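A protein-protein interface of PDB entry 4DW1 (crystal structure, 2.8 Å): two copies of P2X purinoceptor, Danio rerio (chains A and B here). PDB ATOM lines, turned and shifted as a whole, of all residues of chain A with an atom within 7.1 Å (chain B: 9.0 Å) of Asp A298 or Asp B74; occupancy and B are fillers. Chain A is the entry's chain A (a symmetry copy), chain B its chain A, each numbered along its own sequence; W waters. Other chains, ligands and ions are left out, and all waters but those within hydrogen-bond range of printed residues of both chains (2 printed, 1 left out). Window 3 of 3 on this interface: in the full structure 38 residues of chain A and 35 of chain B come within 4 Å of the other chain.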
ATOM      1  N   GLU A  73      11.122 -26.088   8.379  1.00  0.00           N
ATOM      2  CA  GLU A  73      10.033 -26.242   7.414  1.00  0.00           C
ATOM      3  C   GLU A  73       9.617 -27.697   7.335  1.00  0.00           C
ATOM      4  O   GLU A  73      10.410 -28.590   7.573  1.00  0.00           O
ATOM      5  CB  GLU A  73      10.361 -25.736   6.006  1.00  0.00           C
ATOM      6  CG  GLU A  73      11.716 -25.126   5.755  1.00  0.00           C
ATOM      7  CD  GLU A  73      11.864 -24.736   4.279  1.00  0.00           C
ATOM      8  OE1 GLU A  73      13.014 -24.578   3.778  1.00  0.00           O
ATOM      9  OE2 GLU A  73      10.801 -24.594   3.613  1.00  0.00           O
ATOM     10  N   ASP A  74       8.376 -27.935   6.962  1.00  0.00           N
ATOM     11  CA  ASP A  74       7.833 -29.270   7.043  1.00  0.00           C
ATOM     12  C   ASP A  74       8.100 -29.974   5.725  1.00  0.00           C
ATOM     13  O   ASP A  74       7.493 -29.656   4.706  1.00  0.00           O
ATOM     14  CB  ASP A  74       6.334 -29.152   7.310  1.00  0.00           C
ATOM     15  CG  ASP A  74       5.578 -30.430   7.027  1.00  0.00           C
ATOM     16  OD1 ASP A  74       4.356 -30.341   6.750  1.00  0.00           O
ATOM     17  OD2 ASP A  74       6.188 -31.518   7.095  1.00  0.00           O
ATOM     18  N   GLY A  75       9.012 -30.940   5.746  1.00  0.00           N
ATOM     19  CA  GLY A  75       9.340 -31.691   4.544  1.00  0.00           C
ATOM     20  C   GLY A  75      10.342 -31.067   3.577  1.00  0.00           C
ATOM     21  O   GLY A  75      10.431 -31.485   2.422  1.00  0.00           O
ATOM     22  N   SER A  76      11.063 -30.042   4.015  1.00  0.00           N
ATOM     23  CA  SER A  76      12.132 -29.476   3.210  1.00  0.00           C
ATOM     24  C   SER A  76      13.074 -28.625   4.051  1.00  0.00           C
ATOM     25  O   SER A  76      12.753 -28.249   5.181  1.00  0.00           O
ATOM     26  CB  SER A  76      11.567 -28.677   2.032  1.00  0.00           C
ATOM     27  OG  SER A  76      11.513 -27.301   2.328  1.00  0.00           O
ATOM     28  N   PHE A  77      14.251 -28.348   3.508  1.00  0.00           N
ATOM     29  CA  PHE A  77      15.180 -27.423   4.146  1.00  0.00           C
ATOM     30  C   PHE A  77      15.975 -26.688   3.074  1.00  0.00           C
ATOM     31  O   PHE A  77      16.178 -27.204   1.976  1.00  0.00           O
ATOM     32  CB  PHE A  77      16.099 -28.139   5.146  1.00  0.00           C
ATOM     33  CG  PHE A  77      16.889 -29.278   4.553  1.00  0.00           C
ATOM     34  CD1 PHE A  77      18.232 -29.121   4.238  1.00  0.00           C
ATOM     35  CD2 PHE A  77      16.293 -30.509   4.314  1.00  0.00           C
ATOM     36  CE1 PHE A  77      18.963 -30.173   3.699  1.00  0.00           C
ATOM     37  CE2 PHE A  77      17.015 -31.565   3.767  1.00  0.00           C
ATOM     38  CZ  PHE A  77      18.348 -31.401   3.470  1.00  0.00           C
ATOM     39  N   VAL A 230      17.317 -26.722  -6.866  1.00  0.00           N
ATOM     40  CA  VAL A 230      16.383 -27.531  -6.079  1.00  0.00           C
ATOM     41  C   VAL A 230      16.649 -29.037  -6.179  1.00  0.00           C
ATOM     42  O   VAL A 230      16.652 -29.598  -7.269  1.00  0.00           O
ATOM     43  CB  VAL A 230      14.904 -27.239  -6.463  1.00  0.00           C
ATOM     44  CG1 VAL A 230      13.968 -28.226  -5.796  1.00  0.00           C
ATOM     45  CG2 VAL A 230      14.543 -25.848  -6.061  1.00  0.00           C
ATOM     46  N   MET A 231      16.854 -29.680  -5.031  1.00  0.00           N
ATOM     47  CA  MET A 231      17.145 -31.115  -4.968  1.00  0.00           C
ATOM     48  C   MET A 231      16.025 -31.872  -4.299  1.00  0.00           C
ATOM     49  O   MET A 231      15.587 -31.517  -3.200  1.00  0.00           O
ATOM     50  CB  MET A 231      18.444 -31.398  -4.200  1.00  0.00           C
ATOM     51  CG  MET A 231      19.710 -31.007  -4.939  1.00  0.00           C
ATOM     52  SD  MET A 231      19.885 -31.915  -6.492  1.00  0.00           S
ATOM     53  CE  MET A 231      19.678 -33.605  -5.907  1.00  0.00           C
ATOM     54  N   GLY A 232      15.496 -32.855  -5.017  1.00  0.00           N
ATOM     55  CA  GLY A 232      14.647 -33.884  -4.449  1.00  0.00           C
ATOM     56  C   GLY A 232      15.358 -35.021  -3.737  1.00  0.00           C
ATOM     57  O   GLY A 232      16.285 -35.646  -4.280  1.00  0.00           O
ATOM     58  N   VAL A 233      14.870 -35.337  -2.544  1.00  0.00           N
ATOM     59  CA  VAL A 233      15.293 -36.519  -1.818  1.00  0.00           C
ATOM     60  C   VAL A 233      14.065 -37.413  -1.666  1.00  0.00           C
ATOM     61  O   VAL A 233      13.118 -37.061  -0.968  1.00  0.00           O
ATOM     62  CB  VAL A 233      15.825 -36.125  -0.430  1.00  0.00           C
ATOM     63  CG1 VAL A 233      16.090 -37.363   0.439  1.00  0.00           C
ATOM     64  CG2 VAL A 233      17.072 -35.241  -0.575  1.00  0.00           C
ATOM     65  N   GLN A 234      14.060 -38.558  -2.338  1.00  0.00           N
ATOM     66  CA  GLN A 234      12.904 -39.446  -2.280  1.00  0.00           C
ATOM     67  C   GLN A 234      13.166 -40.628  -1.356  1.00  0.00           C
ATOM     68  O   GLN A 234      14.209 -41.284  -1.439  1.00  0.00           O
ATOM     69  CB  GLN A 234      12.517 -39.927  -3.676  1.00  0.00           C
ATOM     70  CG  GLN A 234      13.202 -39.143  -4.814  1.00  0.00           C
ATOM     71  CD  GLN A 234      12.481 -39.276  -6.163  1.00  0.00           C
ATOM     72  OE1 GLN A 234      11.348 -39.757  -6.227  1.00  0.00           O
ATOM     73  NE2 GLN A 234      13.140 -38.842  -7.243  1.00  0.00           N
ATOM     74  N   ARG A 255      17.088 -36.811  -6.878  1.00  0.00           N
ATOM     75  CA  ARG A 255      16.882 -36.260  -8.213  1.00  0.00           C
ATOM     76  C   ARG A 255      17.066 -34.737  -8.148  1.00  0.00           C
ATOM     77  O   ARG A 255      16.833 -34.152  -7.108  1.00  0.00           O
ATOM     78  CB  ARG A 255      15.481 -36.648  -8.713  1.00  0.00           C
ATOM     79  N   LEU A 257      15.386 -31.319  -9.110  1.00  0.00           N
ATOM     80  CA  LEU A 257      14.023 -30.918  -9.452  1.00  0.00           C
ATOM     81  C   LEU A 257      13.883 -29.813 -10.488  1.00  0.00           C
ATOM     82  O   LEU A 257      12.974 -29.843 -11.307  1.00  0.00           O
ATOM     83  CB  LEU A 257      13.270 -30.537  -8.188  1.00  0.00           C
ATOM     84  CG  LEU A 257      13.195 -31.738  -7.261  1.00  0.00           C
ATOM     85  CD1 LEU A 257      12.354 -31.416  -6.056  1.00  0.00           C
ATOM     86  CD2 LEU A 257      12.631 -32.900  -8.030  1.00  0.00           C
ATOM     87  N   TYR A 270      18.086 -20.846  -7.712  1.00  0.00           N
ATOM     88  CA  TYR A 270      17.170 -20.447  -6.657  1.00  0.00           C
ATOM     89  C   TYR A 270      17.817 -19.345  -5.839  1.00  0.00           C
ATOM     90  O   TYR A 270      18.934 -19.511  -5.331  1.00  0.00           O
ATOM     91  CB  TYR A 270      16.882 -21.638  -5.747  1.00  0.00           C
ATOM     92  CG  TYR A 270      15.741 -21.435  -4.788  1.00  0.00           C
ATOM     93  CD1 TYR A 270      14.732 -20.530  -5.055  1.00  0.00           C
ATOM     94  CD2 TYR A 270      15.676 -22.139  -3.611  1.00  0.00           C
ATOM     95  CE1 TYR A 270      13.671 -20.349  -4.159  1.00  0.00           C
ATOM     96  CE2 TYR A 270      14.652 -21.966  -2.719  1.00  0.00           C
ATOM     97  CZ  TYR A 270      13.648 -21.083  -2.988  1.00  0.00           C
ATOM     98  OH  TYR A 270      12.609 -20.935  -2.084  1.00  0.00           O
ATOM     99  N   ILE A 295      20.501 -24.236  -2.139  1.00  0.00           N
ATOM    100  CA  ILE A 295      19.746 -25.374  -2.600  1.00  0.00           C
ATOM    101  C   ILE A 295      18.623 -25.669  -1.634  1.00  0.00           C
ATOM    102  O   ILE A 295      18.832 -25.777  -0.422  1.00  0.00           O
ATOM    103  CB  ILE A 295      20.625 -26.604  -2.768  1.00  0.00           C
ATOM    104  CG1 ILE A 295      21.612 -26.374  -3.918  1.00  0.00           C
ATOM    105  CG2 ILE A 295      19.756 -27.825  -3.067  1.00  0.00           C
ATOM    106  CD1 ILE A 295      23.035 -26.645  -3.574  1.00  0.00           C
ATOM    107  N   ARG A 296      17.417 -25.751  -2.182  1.00  0.00           N
ATOM    108  CA  ARG A 296      16.284 -26.255  -1.439  1.00  0.00           C
ATOM    109  C   ARG A 296      16.313 -27.788  -1.518  1.00  0.00           C
ATOM    110  O   ARG A 296      16.285 -28.380  -2.595  1.00  0.00           O
ATOM    111  CB  ARG A 296      14.989 -25.716  -2.034  1.00  0.00           C
ATOM    112  CG  ARG A 296      13.970 -25.328  -0.999  1.00  0.00           C
ATOM    113  CD  ARG A 296      12.630 -25.950  -1.259  1.00  0.00           C
ATOM    114  NE  ARG A 296      11.963 -25.310  -2.370  1.00  0.00           N
ATOM    115  CZ  ARG A 296      11.271 -25.972  -3.295  1.00  0.00           C
ATOM    116  NH1 ARG A 296      11.164 -27.307  -3.222  1.00  0.00           N
ATOM    117  NH2 ARG A 296      10.692 -25.303  -4.296  1.00  0.00           N
ATOM    118  N   PHE A 297      16.399 -28.448  -0.384  1.00  0.00           N
ATOM    119  CA  PHE A 297      16.297 -29.891  -0.406  1.00  0.00           C
ATOM    120  C   PHE A 297      14.898 -30.224   0.022  1.00  0.00           C
ATOM    121  O   PHE A 297      14.439 -29.850   1.097  1.00  0.00           O
ATOM    122  CB  PHE A 297      17.311 -30.544   0.520  1.00  0.00           C
ATOM    123  CG  PHE A 297      18.717 -30.370   0.068  1.00  0.00           C
ATOM    124  CD1 PHE A 297      19.383 -29.173   0.280  1.00  0.00           C
ATOM    125  CD2 PHE A 297      19.373 -31.397  -0.582  1.00  0.00           C
ATOM    126  CE1 PHE A 297      20.681 -29.006  -0.150  1.00  0.00           C
ATOM    127  CE2 PHE A 297      20.667 -31.242  -1.020  1.00  0.00           C
ATOM    128  CZ  PHE A 297      21.329 -30.050  -0.801  1.00  0.00           C
ATOM    129  N   ASP A 298      14.231 -30.949  -0.845  1.00  0.00           N
ATOM    130  CA  ASP A 298      12.843 -31.250  -0.690  1.00  0.00           C
ATOM    131  C   ASP A 298      12.720 -32.719  -0.371  1.00  0.00           C
ATOM    132  O   ASP A 298      13.208 -33.560  -1.124  1.00  0.00           O
ATOM    133  CB  ASP A 298      12.192 -30.979  -2.027  1.00  0.00           C
ATOM    134  CG  ASP A 298      10.760 -30.660  -1.899  1.00  0.00           C
ATOM    135  OD1 ASP A 298      10.452 -29.442  -1.831  1.00  0.00           O
ATOM    136  OD2 ASP A 298       9.963 -31.631  -1.857  1.00  0.00           O
ATOM    137  N   VAL A 299      12.077 -33.054   0.735  1.00  0.00           N
ATOM    138  CA  VAL A 299      11.998 -34.462   1.097  1.00  0.00           C
ATOM    139  C   VAL A 299      10.633 -35.043   0.793  1.00  0.00           C
ATOM    140  O   VAL A 299       9.625 -34.518   1.224  1.00  0.00           O
ATOM    141  CB  VAL A 299      12.361 -34.719   2.554  1.00  0.00           C
ATOM    142  CG1 VAL A 299      12.402 -36.214   2.803  1.00  0.00           C
ATOM    143  CG2 VAL A 299      13.701 -34.095   2.882  1.00  0.00           C
ATOM    144  N   MET A 300      10.627 -36.142   0.049  1.00  0.00           N
ATOM    145  CA  MET A 300       9.403 -36.749  -0.446  1.00  0.00           C
ATOM    146  C   MET A 300       9.340 -38.219  -0.061  1.00  0.00           C
ATOM    147  O   MET A 300      10.239 -38.996  -0.382  1.00  0.00           O
ATOM    148  CB  MET A 300       9.339 -36.613  -1.966  1.00  0.00           C
ATOM    149  CG  MET A 300       9.245 -35.170  -2.440  1.00  0.00           C
ATOM    150  SD  MET A 300       9.693 -34.910  -4.173  1.00  0.00           S
ATOM    151  CE  MET A 300      11.457 -35.275  -4.144  1.00  0.00           C
ATOM    152  N   SER B  40       6.108 -31.802  -9.943  1.00  0.00           N
ATOM    153  CA  SER B  40       6.202 -30.358 -10.039  1.00  0.00           C
ATOM    154  C   SER B  40       7.061 -29.750  -8.949  1.00  0.00           C
ATOM    155  O   SER B  40       7.154 -30.273  -7.845  1.00  0.00           O
ATOM    156  CB  SER B  40       4.799 -29.764  -9.950  1.00  0.00           C
ATOM    157  OG  SER B  40       4.860 -28.360  -9.862  1.00  0.00           O
ATOM    158  N   SER B  41       7.684 -28.626  -9.264  1.00  0.00           N
ATOM    159  CA  SER B  41       8.415 -27.851  -8.272  1.00  0.00           C
ATOM    160  C   SER B  41       8.312 -26.355  -8.582  1.00  0.00           C
ATOM    161  O   SER B  41       8.439 -25.946  -9.731  1.00  0.00           O
ATOM    162  CB  SER B  41       9.874 -28.287  -8.246  1.00  0.00           C
ATOM    163  OG  SER B  41      10.658 -27.286  -7.629  1.00  0.00           O
ATOM    164  N   VAL B  42       8.093 -25.523  -7.571  1.00  0.00           N
ATOM    165  CA  VAL B  42       8.003 -24.094  -7.849  1.00  0.00           C
ATOM    166  C   VAL B  42       8.827 -23.230  -6.916  1.00  0.00           C
ATOM    167  O   VAL B  42       8.981 -23.545  -5.746  1.00  0.00           O
ATOM    168  CB  VAL B  42       6.525 -23.573  -7.921  1.00  0.00           C
ATOM    169  CG1 VAL B  42       5.546 -24.713  -7.960  1.00  0.00           C
ATOM    170  CG2 VAL B  42       6.222 -22.672  -6.772  1.00  0.00           C
ATOM    171  N   THR B  43       9.362 -22.138  -7.457  1.00  0.00           N
ATOM    172  CA  THR B  43       9.978 -21.094  -6.645  1.00  0.00           C
ATOM    173  C   THR B  43       9.323 -19.786  -7.067  1.00  0.00           C
ATOM    174  O   THR B  43       8.794 -19.698  -8.176  1.00  0.00           O
ATOM    175  CB  THR B  43      11.510 -21.047  -6.808  1.00  0.00           C
ATOM    176  OG1 THR B  43      11.845 -20.616  -8.120  1.00  0.00           O
ATOM    177  CG2 THR B  43      12.084 -22.420  -6.633  1.00  0.00           C
ATOM    178  N   THR B  44       9.317 -18.796  -6.177  1.00  0.00           N
ATOM    179  CA  THR B  44       8.667 -17.531  -6.459  1.00  0.00           C
ATOM    180  C   THR B  44       9.505 -16.349  -5.989  1.00  0.00           C
ATOM    181  O   THR B  44      10.328 -16.471  -5.094  1.00  0.00           O
ATOM    182  CB  THR B  44       7.302 -17.458  -5.793  1.00  0.00           C
ATOM    183  OG1 THR B  44       7.465 -17.666  -4.390  1.00  0.00           O
ATOM    184  CG2 THR B  44       6.371 -18.529  -6.342  1.00  0.00           C
ATOM    185  N   PRO B  70       7.594 -15.749   5.791  1.00  0.00           N
ATOM    186  CA  PRO B  70       9.047 -15.618   5.762  1.00  0.00           C
ATOM    187  C   PRO B  70       9.522 -15.459   4.316  1.00  0.00           C
ATOM    188  O   PRO B  70       8.708 -15.455   3.393  1.00  0.00           O
ATOM    189  CB  PRO B  70       9.501 -16.951   6.355  1.00  0.00           C
ATOM    190  CG  PRO B  70       8.454 -17.915   5.946  1.00  0.00           C
ATOM    191  CD  PRO B  70       7.166 -17.154   5.920  1.00  0.00           C
ATOM    192  N   PRO B  71      10.838 -15.338   4.111  1.00  0.00           N
ATOM    193  CA  PRO B  71      11.367 -15.061   2.776  1.00  0.00           C
ATOM    194  C   PRO B  71      11.126 -16.206   1.816  1.00  0.00           C
ATOM    195  O   PRO B  71      11.109 -16.005   0.606  1.00  0.00           O
ATOM    196  CB  PRO B  71      12.867 -14.958   3.024  1.00  0.00           C
ATOM    197  CG  PRO B  71      13.010 -14.739   4.489  1.00  0.00           C
ATOM    198  CD  PRO B  71      11.908 -15.482   5.105  1.00  0.00           C
ATOM    199  N   GLN B  72      10.994 -17.407   2.358  1.00  0.00           N
ATOM    200  CA  GLN B  72      11.058 -18.623   1.556  1.00  0.00           C
ATOM    201  C   GLN B  72      10.035 -19.639   2.054  1.00  0.00           C
ATOM    202  O   GLN B  72      10.049 -20.005   3.222  1.00  0.00           O
ATOM    203  CB  GLN B  72      12.482 -19.180   1.694  1.00  0.00           C
ATOM    204  CG  GLN B  72      12.852 -20.302   0.789  1.00  0.00           C
ATOM    205  CD  GLN B  72      12.778 -21.632   1.478  1.00  0.00           C
ATOM    206  OE1 GLN B  72      13.304 -21.807   2.581  1.00  0.00           O
ATOM    207  NE2 GLN B  72      12.105 -22.580   0.842  1.00  0.00           N
ATOM    208  N   GLU B  73       9.131 -20.078   1.190  1.00  0.00           N
ATOM    209  CA  GLU B  73       8.290 -21.231   1.510  1.00  0.00           C
ATOM    210  C   GLU B  73       8.051 -22.057   0.263  1.00  0.00           C
ATOM    211  O   GLU B  73       8.063 -21.543  -0.841  1.00  0.00           O
ATOM    212  CB  GLU B  73       6.940 -20.872   2.141  1.00  0.00           C
ATOM    213  CG  GLU B  73       6.622 -19.421   2.389  1.00  0.00           C
ATOM    214  CD  GLU B  73       5.209 -19.273   2.971  1.00  0.00           C
ATOM    215  OE1 GLU B  73       4.605 -18.167   2.890  1.00  0.00           O
ATOM    216  OE2 GLU B  73       4.702 -20.294   3.512  1.00  0.00           O
ATOM    217  N   ASP B  74       7.797 -23.337   0.444  1.00  0.00           N
ATOM    218  CA  ASP B  74       7.749 -24.237  -0.683  1.00  0.00           C
ATOM    219  C   ASP B  74       6.321 -24.283  -1.196  1.00  0.00           C
ATOM    220  O   ASP B  74       5.438 -24.843  -0.553  1.00  0.00           O
ATOM    221  CB  ASP B  74       8.207 -25.614  -0.206  1.00  0.00           C
ATOM    222  CG  ASP B  74       7.834 -26.727  -1.158  1.00  0.00           C
ATOM    223  OD1 ASP B  74       7.719 -27.887  -0.689  1.00  0.00           O
ATOM    224  OD2 ASP B  74       7.671 -26.457  -2.367  1.00  0.00           O
ATOM    225  N   GLY B  75       6.094 -23.692  -2.364  1.00  0.00           N
ATOM    226  CA  GLY B  75       4.766 -23.684  -2.958  1.00  0.00           C
ATOM    227  C   GLY B  75       3.787 -22.617  -2.477  1.00  0.00           C
ATOM    228  O   GLY B  75       2.582 -22.738  -2.699  1.00  0.00           O
ATOM    229  N   SER B  76       4.280 -21.600  -1.782  1.00  0.00           N
ATOM    230  CA  SER B  76       3.444 -20.474  -1.402  1.00  0.00           C
ATOM    231  C   SER B  76       4.282 -19.266  -1.002  1.00  0.00           C
ATOM    232  O   SER B  76       5.484 -19.381  -0.752  1.00  0.00           O
ATOM    233  CB  SER B  76       2.469 -20.865  -0.288  1.00  0.00           C
ATOM    234  OG  SER B  76       2.965 -20.495   0.977  1.00  0.00           O
ATOM    235  N   PHE B  77       3.648 -18.102  -0.970  1.00  0.00           N
ATOM    236  CA  PHE B  77       4.298 -16.901  -0.460  1.00  0.00           C
ATOM    237  C   PHE B  77       3.257 -16.007   0.200  1.00  0.00           C
ATOM    238  O   PHE B  77       2.079 -16.042  -0.154  1.00  0.00           O
ATOM    239  CB  PHE B  77       5.067 -16.160  -1.563  1.00  0.00           C
ATOM    240  CG  PHE B  77       4.227 -15.780  -2.755  1.00  0.00           C
ATOM    241  CD1 PHE B  77       3.781 -14.477  -2.922  1.00  0.00           C
ATOM    242  CD2 PHE B  77       3.886 -16.725  -3.715  1.00  0.00           C
ATOM    243  CE1 PHE B  77       3.013 -14.124  -4.025  1.00  0.00           C
ATOM    244  CE2 PHE B  77       3.110 -16.382  -4.818  1.00  0.00           C
ATOM    245  CZ  PHE B  77       2.684 -15.085  -4.978  1.00  0.00           C
ATOM    246  N   ARG B 296      -1.944 -14.738   1.595  1.00  0.00           N
ATOM    247  CA  ARG B 296      -1.151 -15.912   1.301  1.00  0.00           C
ATOM    248  C   ARG B 296      -1.454 -16.337  -0.143  1.00  0.00           C
ATOM    249  O   ARG B 296      -2.593 -16.614  -0.509  1.00  0.00           O
ATOM    250  CB  ARG B 296      -1.504 -17.035   2.271  1.00  0.00           C
ATOM    251  CG  ARG B 296      -0.311 -17.818   2.740  1.00  0.00           C
ATOM    252  CD  ARG B 296      -0.497 -19.297   2.566  1.00  0.00           C
ATOM    253  NE  ARG B 296      -1.416 -19.828   3.545  1.00  0.00           N
ATOM    254  CZ  ARG B 296      -2.338 -20.748   3.269  1.00  0.00           C
ATOM    255  NH1 ARG B 296      -2.447 -21.232   2.023  1.00  0.00           N
ATOM    256  NH2 ARG B 296      -3.157 -21.178   4.233  1.00  0.00           N
ATOM    257  N   PHE B 297      -0.445 -16.364  -0.985  1.00  0.00           N
ATOM    258  CA  PHE B 297      -0.662 -16.883  -2.319  1.00  0.00           C
ATOM    259  C   PHE B 297      -0.124 -18.283  -2.323  1.00  0.00           C
ATOM    260  O   PHE B 297       1.040 -18.534  -2.027  1.00  0.00           O
ATOM    261  CB  PHE B 297       0.032 -16.039  -3.375  1.00  0.00           C
ATOM    262  CG  PHE B 297      -0.554 -14.679  -3.520  1.00  0.00           C
ATOM    263  CD1 PHE B 297      -0.252 -13.681  -2.607  1.00  0.00           C
ATOM    264  CD2 PHE B 297      -1.417 -14.399  -4.559  1.00  0.00           C
ATOM    265  CE1 PHE B 297      -0.803 -12.425  -2.732  1.00  0.00           C
ATOM    266  CE2 PHE B 297      -1.979 -13.151  -4.693  1.00  0.00           C
ATOM    267  CZ  PHE B 297      -1.670 -12.157  -3.785  1.00  0.00           C
ATOM    268  N   ASP B 298      -1.001 -19.194  -2.675  1.00  0.00           N
ATOM    269  CA  ASP B 298      -0.728 -20.595  -2.604  1.00  0.00           C
ATOM    270  C   ASP B 298      -0.612 -21.116  -4.015  1.00  0.00           C
ATOM    271  O   ASP B 298      -1.531 -20.949  -4.815  1.00  0.00           O
ATOM    272  CB  ASP B 298      -1.925 -21.233  -1.938  1.00  0.00           C
ATOM    273  CG  ASP B 298      -1.583 -22.497  -1.265  1.00  0.00           C
ATOM    274  OD1 ASP B 298      -1.304 -22.432  -0.039  1.00  0.00           O
ATOM    275  OD2 ASP B 298      -1.587 -23.537  -1.970  1.00  0.00           O
ATOM    276  N   VAL B 299       0.503 -21.746  -4.345  1.00  0.00           N
ATOM    277  CA  VAL B 299       0.664 -22.205  -5.717  1.00  0.00           C
ATOM    278  C   VAL B 299       0.444 -23.699  -5.839  1.00  0.00           C
ATOM    279  O   VAL B 299       1.063 -24.476  -5.139  1.00  0.00           O
ATOM    280  CB  VAL B 299       2.015 -21.827  -6.310  1.00  0.00           C
ATOM    281  CG1 VAL B 299       2.039 -22.206  -7.779  1.00  0.00           C
ATOM    282  CG2 VAL B 299       2.269 -20.344  -6.146  1.00  0.00           C
ATOM    283  N   MET B 300      -0.445 -24.078  -6.748  1.00  0.00           N
ATOM    284  CA  MET B 300      -0.874 -25.457  -6.900  1.00  0.00           C
ATOM    285  C   MET B 300      -0.700 -25.917  -8.340  1.00  0.00           C
ATOM    286  O   MET B 300      -1.234 -25.309  -9.266  1.00  0.00           O
ATOM    287  CB  MET B 300      -2.339 -25.589  -6.492  1.00  0.00           C
ATOM    288  CG  MET B 300      -2.586 -25.293  -5.020  1.00  0.00           C
ATOM    289  SD  MET B 300      -4.305 -24.916  -4.599  1.00  0.00           S
ATOM    290  CE  MET B 300      -4.538 -23.337  -5.435  1.00  0.00           C
ATOM    291  N   VAL B 301       0.051 -26.999  -8.511  1.00  0.00           N
ATOM    292  CA  VAL B 301       0.322 -27.562  -9.824  1.00  0.00           C
ATOM    293  C   VAL B 301      -0.323 -28.943  -9.988  1.00  0.00           C
ATOM    294  O   VAL B 301      -0.114 -29.839  -9.165  1.00  0.00           O
ATOM    295  CB  VAL B 301       1.828 -27.681 -10.055  1.00  0.00           C
ATOM    296  CG1 VAL B 301       2.110 -28.068 -11.496  1.00  0.00           C
ATOM    297  CG2 VAL B 301       2.511 -26.384  -9.714  1.00  0.00           C
HETATM  298  O   HOH W   1      11.156 -25.106   1.054  1.00  0.00           O
HETATM  299  O   HOH W   2      10.280 -19.302  -3.037  1.00  0.00           O
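OE1 of Gln B72 lies close to OE1 of Glu A73 (3.0 Å).
NE2 of Gln B72 sits close to OH of Tyr A270 (3.4 Å).
NH2 of Arg A296 lies within hydrogen-bond range of O of Val B42 (2.8 Å).
The guanidinium group (NH1) of Arg A296 lies within salt-bridge range of the side-chain carboxylate (OD2) of Asp B74 (3.7 Å).
The side-chain carboxylate (OD1) of Asp A298 lies close to the side-chain carboxylate (OD1) of Asp B74 (3.3 Å).
N of Asp A298 sits at hydrogen-bond distance from O of Met A231, 2.8 Å away.
The side-chain carboxylate of Asp A298 lies within salt-bridge range of the guanidinium group of Arg A296 (2.6 Å).
N of Met A231 lies within hydrogen-bond range of O of Arg A296, 2.8 Å away.
The backbone NH of Val A233 sits at hydrogen-bond distance from the backbone carbonyl oxygen of Asp A298 (2.8 Å).
The backbone carbonyl oxygen (O) of Val A230 sits at hydrogen-bond distance from the backbone NH (N) of Leu A257.
OG of Ser A76 sits at hydrogen-bond distance from OE2 of Glu A73 (3.1 Å).
Among the printed residues, pairs that only touch across the chains: Tyr A270 with Thr B43 (3.5 Å), Arg A296 with Gln B72 (3.8 Å), Arg A296 with Ser B41 (3.9 Å), Val A230 with Ser B41 (3.9 Å) and Arg A296 with Thr B43 (3.96 Å).
Printed residues of chain B within 4 Å of Glu A73: Gln B72.
Asp A298 touches just one residue of chain B: Asp B74 (3.3 Å).
No residue of chain B comes within 4 Å of Val A299.
Of the printed residues of chain A, Val B42 touches Arg A296.
Of the printed residues of chain A, Gln B72 touches Glu A73 (3.0 Å), Tyr A270 (3.0 Å) and Arg A296 (3.8 Å).
The nearest residue of chain A that does not touch Asp B74 is Ser A76 (4.5 Å).
Hydrophobic or aromatic side chains of chain A within 4 Å of the printed part of chain B: Val A230 and Tyr A270.
Arg A296 touches Asp B74, but with the chains exchanged Asp A74 does not touch Arg B296 (12.1 Å).
Asp A298 touches Asp B74, but with the chains exchanged Asp A74 does not touch Asp B298 (11.9 Å).
Positions printed for both chains: 73, 74, 75, 76, 77, 296, 297, 298, 299 and 300.
Of the 10 pairs that touch across the chains among the printed residues, none has its exchanged pair printed and touching as well.
Water W1 lies within hydrogen-bond range of OG of Ser A76 (2.6 Å), OE2 of Glu A73 (2.6 Å) and NE2 of Gln B72 (2.7 Å).
Water W2 lies within hydrogen-bond range of OH of Tyr A270 (3.0 Å) and N of Thr B44 (3.3 Å).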
